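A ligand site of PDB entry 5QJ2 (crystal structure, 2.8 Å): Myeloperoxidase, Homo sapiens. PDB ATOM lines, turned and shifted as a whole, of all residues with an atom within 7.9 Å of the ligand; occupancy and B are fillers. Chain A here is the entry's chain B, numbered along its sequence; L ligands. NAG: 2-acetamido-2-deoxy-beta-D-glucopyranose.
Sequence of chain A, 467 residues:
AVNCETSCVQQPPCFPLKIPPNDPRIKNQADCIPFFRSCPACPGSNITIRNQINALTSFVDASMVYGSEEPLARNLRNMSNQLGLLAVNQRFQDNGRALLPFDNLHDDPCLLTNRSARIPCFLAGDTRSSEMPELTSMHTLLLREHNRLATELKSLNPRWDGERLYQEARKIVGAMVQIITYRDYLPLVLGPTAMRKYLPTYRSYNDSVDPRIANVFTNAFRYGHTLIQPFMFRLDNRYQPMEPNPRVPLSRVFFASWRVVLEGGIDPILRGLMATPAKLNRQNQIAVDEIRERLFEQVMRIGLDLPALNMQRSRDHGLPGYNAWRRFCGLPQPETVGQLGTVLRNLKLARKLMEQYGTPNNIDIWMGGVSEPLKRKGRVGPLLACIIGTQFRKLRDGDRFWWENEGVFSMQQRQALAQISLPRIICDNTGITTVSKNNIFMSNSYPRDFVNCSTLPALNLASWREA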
ATOM      1  N   LEU A  76     -27.178   6.076   5.747  1.00  0.00           N
ATOM      2  CA  LEU A  76     -26.398   4.911   5.344  1.00  0.00           C
ATOM      3  C   LEU A  76     -25.894   5.135   3.906  1.00  0.00           C
ATOM      4  O   LEU A  76     -24.864   4.578   3.529  1.00  0.00           O
ATOM      5  CB  LEU A  76     -27.289   3.670   5.405  1.00  0.00           C
ATOM      6  CG  LEU A  76     -26.775   2.448   6.153  1.00  0.00           C
ATOM      7  CD1 LEU A  76     -26.521   2.746   7.604  1.00  0.00           C
ATOM      8  CD2 LEU A  76     -27.798   1.351   6.114  1.00  0.00           C
ATOM      9  N   ARG A  77     -26.620   5.974   3.149  1.00  0.00           N
ATOM     10  CA  ARG A  77     -26.274   6.362   1.785  1.00  0.00           C
ATOM     11  C   ARG A  77     -25.246   7.502   1.824  1.00  0.00           C
ATOM     12  O   ARG A  77     -25.211   8.294   2.777  1.00  0.00           O
ATOM     13  CB  ARG A  77     -27.503   6.878   1.027  1.00  0.00           C
ATOM     14  CG  ARG A  77     -28.554   5.832   0.712  1.00  0.00           C
ATOM     15  CD  ARG A  77     -29.798   6.489   0.153  1.00  0.00           C
ATOM     16  NE  ARG A  77     -29.701   6.767  -1.285  1.00  0.00           N
ATOM     17  CZ  ARG A  77     -30.588   7.469  -1.980  1.00  0.00           C
ATOM     18  NH1 ARG A  77     -31.629   8.015  -1.376  1.00  0.00           N
ATOM     19  NH2 ARG A  77     -30.432   7.639  -3.283  1.00  0.00           N
ATOM     20  N   ASN A  78     -24.437   7.579   0.752  1.00  0.00           N
ATOM     21  CA  ASN A  78     -23.457   8.626   0.519  1.00  0.00           C
ATOM     22  C   ASN A  78     -24.230   9.742  -0.191  1.00  0.00           C
ATOM     23  O   ASN A  78     -24.476   9.667  -1.405  1.00  0.00           O
ATOM     24  CB  ASN A  78     -22.297   8.109  -0.340  1.00  0.00           C
ATOM     25  CG  ASN A  78     -21.163   9.099  -0.531  1.00  0.00           C
ATOM     26  OD1 ASN A  78     -21.080  10.151   0.106  1.00  0.00           O
ATOM     27  ND2 ASN A  78     -20.199   8.716  -1.362  1.00  0.00           N
ATOM     28  N   MET A  79     -24.679  10.724   0.587  1.00  0.00           N
ATOM     29  CA  MET A  79     -25.509  11.833   0.104  1.00  0.00           C
ATOM     30  C   MET A  79     -24.725  12.989  -0.538  1.00  0.00           C
ATOM     31  O   MET A  79     -25.327  13.832  -1.211  1.00  0.00           O
ATOM     32  CB  MET A  79     -26.417  12.328   1.245  1.00  0.00           C
ATOM     33  CG  MET A  79     -27.438  11.296   1.723  1.00  0.00           C
ATOM     34  SD  MET A  79     -28.767  11.005   0.521  1.00  0.00           S
ATOM     35  CE  MET A  79     -29.887  10.074   1.486  1.00  0.00           C
ATOM     36  N   SER A  80     -23.389  13.016  -0.358  1.00  0.00           N
ATOM     37  CA  SER A  80     -22.472  14.047  -0.879  1.00  0.00           C
ATOM     38  C   SER A  80     -22.345  14.096  -2.413  1.00  0.00           C
ATOM     39  O   SER A  80     -21.914  15.118  -2.946  1.00  0.00           O
ATOM     40  CB  SER A  80     -21.106  13.919  -0.230  1.00  0.00           C
ATOM     41  OG  SER A  80     -21.195  14.037   1.182  1.00  0.00           O
ATOM     42  N   ASN A  81     -22.698  13.009  -3.120  1.00  0.00           N
ATOM     43  CA  ASN A  81     -22.611  12.935  -4.579  1.00  0.00           C
ATOM     44  C   ASN A  81     -23.838  12.276  -5.229  1.00  0.00           C
ATOM     45  O   ASN A  81     -24.666  11.687  -4.538  1.00  0.00           O
ATOM     46  CB  ASN A  81     -21.322  12.218  -5.017  1.00  0.00           C
ATOM     47  CG  ASN A  81     -21.025  10.944  -4.273  1.00  0.00           C
ATOM     48  OD1 ASN A  81     -20.237  10.921  -3.310  1.00  0.00           O
ATOM     49  ND2 ASN A  81     -21.670   9.856  -4.674  1.00  0.00           N
ATOM     50  N   LEU A  83     -23.702   9.761  -7.319  1.00  0.00           N
ATOM     51  CA  LEU A  83     -23.218   8.455  -7.754  1.00  0.00           C
ATOM     52  C   LEU A  83     -23.968   7.319  -7.038  1.00  0.00           C
ATOM     53  O   LEU A  83     -23.670   6.131  -7.254  1.00  0.00           O
ATOM     54  CB  LEU A  83     -21.694   8.325  -7.572  1.00  0.00           C
ATOM     55  CG  LEU A  83     -20.828   9.340  -8.318  1.00  0.00           C
ATOM     56  CD1 LEU A  83     -19.544   9.615  -7.567  1.00  0.00           C
ATOM     57  CD2 LEU A  83     -20.524   8.880  -9.721  1.00  0.00           C
ATOM     58  N   LEU A  85     -24.040   5.866  -4.170  1.00  0.00           N
ATOM     59  CA  LEU A  85     -23.359   4.806  -3.422  1.00  0.00           C
ATOM     60  C   LEU A  85     -23.879   4.796  -1.981  1.00  0.00           C
ATOM     61  O   LEU A  85     -24.752   5.594  -1.605  1.00  0.00           O
ATOM     62  CB  LEU A  85     -21.824   5.010  -3.428  1.00  0.00           C
ATOM     63  CG  LEU A  85     -21.191   5.668  -4.646  1.00  0.00           C
ATOM     64  CD1 LEU A  85     -20.331   6.824  -4.235  1.00  0.00           C
ATOM     65  CD2 LEU A  85     -20.378   4.692  -5.443  1.00  0.00           C
ATOM     66  N   LEU A  86     -23.335   3.874  -1.187  1.00  0.00           N
ATOM     67  CA  LEU A  86     -23.608   3.766   0.226  1.00  0.00           C
ATOM     68  C   LEU A  86     -22.384   4.348   0.934  1.00  0.00           C
ATOM     69  O   LEU A  86     -21.248   4.018   0.573  1.00  0.00           O
ATOM     70  CB  LEU A  86     -23.824   2.308   0.671  1.00  0.00           C
ATOM     71  CG  LEU A  86     -25.154   1.642   0.294  1.00  0.00           C
ATOM     72  CD1 LEU A  86     -25.045   0.142   0.465  1.00  0.00           C
ATOM     73  CD2 LEU A  86     -26.310   2.172   1.150  1.00  0.00           C
ATOM     74  N   ALA A  87     -22.614   5.221   1.922  1.00  0.00           N
ATOM     75  CA  ALA A  87     -21.568   5.849   2.723  1.00  0.00           C
ATOM     76  C   ALA A  87     -20.630   4.793   3.325  1.00  0.00           C
ATOM     77  O   ALA A  87     -21.015   3.624   3.482  1.00  0.00           O
ATOM     78  CB  ALA A  87     -22.189   6.697   3.825  1.00  0.00           C
ATOM     79  N   VAL A  88     -19.378   5.174   3.584  1.00  0.00           N
ATOM     80  CA  VAL A  88     -18.327   4.274   4.076  1.00  0.00           C
ATOM     81  C   VAL A  88     -17.573   4.890   5.269  1.00  0.00           C
ATOM     82  O   VAL A  88     -17.858   6.039   5.648  1.00  0.00           O
ATOM     83  CB  VAL A  88     -17.369   3.833   2.938  1.00  0.00           C
ATOM     84  CG1 VAL A  88     -18.031   2.792   2.029  1.00  0.00           C
ATOM     85  CG2 VAL A  88     -16.862   5.032   2.121  1.00  0.00           C
ATOM     86  N   ASN A  89     -16.633   4.115   5.861  1.00  0.00           N
ATOM     87  CA  ASN A  89     -15.815   4.579   6.982  1.00  0.00           C
ATOM     88  C   ASN A  89     -14.824   5.624   6.487  1.00  0.00           C
ATOM     89  O   ASN A  89     -14.004   5.339   5.606  1.00  0.00           O
ATOM     90  CB  ASN A  89     -15.068   3.414   7.597  1.00  0.00           C
ATOM     91  CG  ASN A  89     -14.959   3.537   9.085  1.00  0.00           C
ATOM     92  OD1 ASN A  89     -14.019   4.125   9.613  1.00  0.00           O
ATOM     93  ND2 ASN A  89     -15.916   2.964   9.787  1.00  0.00           N
ATOM     94  N   GLN A  90     -14.946   6.861   7.015  1.00  0.00           N
ATOM     95  CA  GLN A  90     -14.084   7.995   6.636  1.00  0.00           C
ATOM     96  C   GLN A  90     -12.816   8.074   7.512  1.00  0.00           C
ATOM     97  O   GLN A  90     -11.928   8.897   7.259  1.00  0.00           O
ATOM     98  CB  GLN A  90     -14.874   9.323   6.636  1.00  0.00           C
ATOM     99  CG  GLN A  90     -16.139   9.349   5.772  1.00  0.00           C
ATOM    100  CD  GLN A  90     -15.882   9.319   4.283  1.00  0.00           C
ATOM    101  OE1 GLN A  90     -15.586  10.338   3.656  1.00  0.00           O
ATOM    102  NE2 GLN A  90     -16.068   8.159   3.676  1.00  0.00           N
ATOM    103  N   GLN A  93      -9.625   2.144   6.429  1.00  0.00           N
ATOM    104  CA  GLN A  93      -9.678   1.399   5.155  1.00  0.00           C
ATOM    105  C   GLN A  93      -9.046   0.003   5.232  1.00  0.00           C
ATOM    106  O   GLN A  93      -8.293  -0.286   6.159  1.00  0.00           O
ATOM    107  CB  GLN A  93      -9.100   2.219   4.001  1.00  0.00           C
ATOM    108  CG  GLN A  93     -10.106   3.125   3.339  1.00  0.00           C
ATOM    109  CD  GLN A  93      -9.546   3.920   2.180  1.00  0.00           C
ATOM    110  OE1 GLN A  93      -8.346   3.916   1.895  1.00  0.00           O
ATOM    111  NE2 GLN A  93     -10.420   4.625   1.480  1.00  0.00           N
ATOM    112  N   PRO A 101     -19.352   2.080   7.706  1.00  0.00           N
ATOM    113  CA  PRO A 101     -19.163   3.255   8.582  1.00  0.00           C
ATOM    114  C   PRO A 101     -19.319   2.982  10.078  1.00  0.00           C
ATOM    115  O   PRO A 101     -19.728   1.900  10.491  1.00  0.00           O
ATOM    116  CB  PRO A 101     -20.200   4.266   8.068  1.00  0.00           C
ATOM    117  CG  PRO A 101     -21.173   3.484   7.270  1.00  0.00           C
ATOM    118  CD  PRO A 101     -20.453   2.289   6.749  1.00  0.00           C
ATOM    119  N   ASN A 147     -21.521  -0.195  -4.141  1.00  0.00           N
ATOM    120  CA  ASN A 147     -20.728   0.913  -4.715  1.00  0.00           C
ATOM    121  C   ASN A 147     -20.073   0.432  -6.027  1.00  0.00           C
ATOM    122  O   ASN A 147     -20.098   1.171  -7.013  1.00  0.00           O
ATOM    123  CB  ASN A 147     -19.680   1.400  -3.716  1.00  0.00           C
ATOM    124  CG  ASN A 147     -20.212   1.903  -2.381  1.00  0.00           C
ATOM    125  OD1 ASN A 147     -21.421   1.917  -2.095  1.00  0.00           O
ATOM    126  ND2 ASN A 147     -19.306   2.345  -1.506  1.00  0.00           N
ATOM    127  N   THR A 151     -21.055   2.182  -9.568  1.00  0.00           N
ATOM    128  CA  THR A 151     -19.985   2.681 -10.443  1.00  0.00           C
ATOM    129  C   THR A 151     -20.149   2.074 -11.853  1.00  0.00           C
ATOM    130  O   THR A 151     -20.302   2.838 -12.818  1.00  0.00           O
ATOM    131  CB  THR A 151     -18.576   2.418  -9.851  1.00  0.00           C
ATOM    132  OG1 THR A 151     -18.550   2.759  -8.467  1.00  0.00           O
ATOM    133  CG2 THR A 151     -17.492   3.197 -10.576  1.00  0.00           C
HETATM  134  C1  NAG L   1     -17.883  10.725  -1.230  1.00  0.00           C
HETATM  135  C2  NAG L   1     -17.283   9.898  -0.063  1.00  0.00           C
HETATM  136  C3  NAG L   1     -15.747  10.161   0.002  1.00  0.00           C
HETATM  137  C4  NAG L   1     -15.058   9.874  -1.379  1.00  0.00           C
HETATM  138  C5  NAG L   1     -16.037   9.922  -2.672  1.00  0.00           C
HETATM  139  C6  NAG L   1     -15.906   8.672  -3.594  1.00  0.00           C
HETATM  140  C7  NAG L   1     -18.723   8.655   1.549  1.00  0.00           C
HETATM  141  C8  NAG L   1     -19.379   8.775   2.892  1.00  0.00           C
HETATM  142  N2  NAG L   1     -18.015   9.787   1.208  1.00  0.00           N
HETATM  143  O3  NAG L   1     -15.199   9.306   1.029  1.00  0.00           O
HETATM  144  O4  NAG L   1     -13.732  10.527  -1.488  1.00  0.00           O
HETATM  145  O5  NAG L   1     -17.490  10.081  -2.455  1.00  0.00           O
HETATM  146  O6  NAG L   1     -16.965   8.554  -4.554  1.00  0.00           O
HETATM  147  O7  NAG L   1     -18.834   7.637   0.819  1.00  0.00           O
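The side-chain amide nitrogen (ND2) of Asn 78 is in hydrogen-bond range of an oxygen (O7) of the ligand, 2.8 Å away.
The side-chain amide oxygen (OE1) of Gln 90 lies within hydrogen-bond range of an oxygen (O3) of the ligand.
The side-chain amide oxygen of Asn 81 lies close to an oxygen (O5) of the ligand (3.0 Å).
ND2 of Asn 78 lies within hydrogen-bond range of OD1 of Asn 81 (2.9 Å).
N of Asn 78 sits at hydrogen-bond distance from O of Leu 85.
O of Val 88 lies within hydrogen-bond range of NE2 of Gln 90, at 3.4 Å.
ND2 of Asn 81 lies close to N of Leu 83, at 3.3 Å.
The backbone carbonyl oxygen (O) of Leu 76 sits at hydrogen-bond distance from the backbone NH (N) of Ala 87 (2.8 Å).
Residues that only touch the ligand: Val 88 (3.5 Å), Ala 87 (3.6 Å) and Leu 85 (3.8 Å).
Hydrophobic or aromatic side chains that line the ligand: Leu 85, Ala 87 and Val 88.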
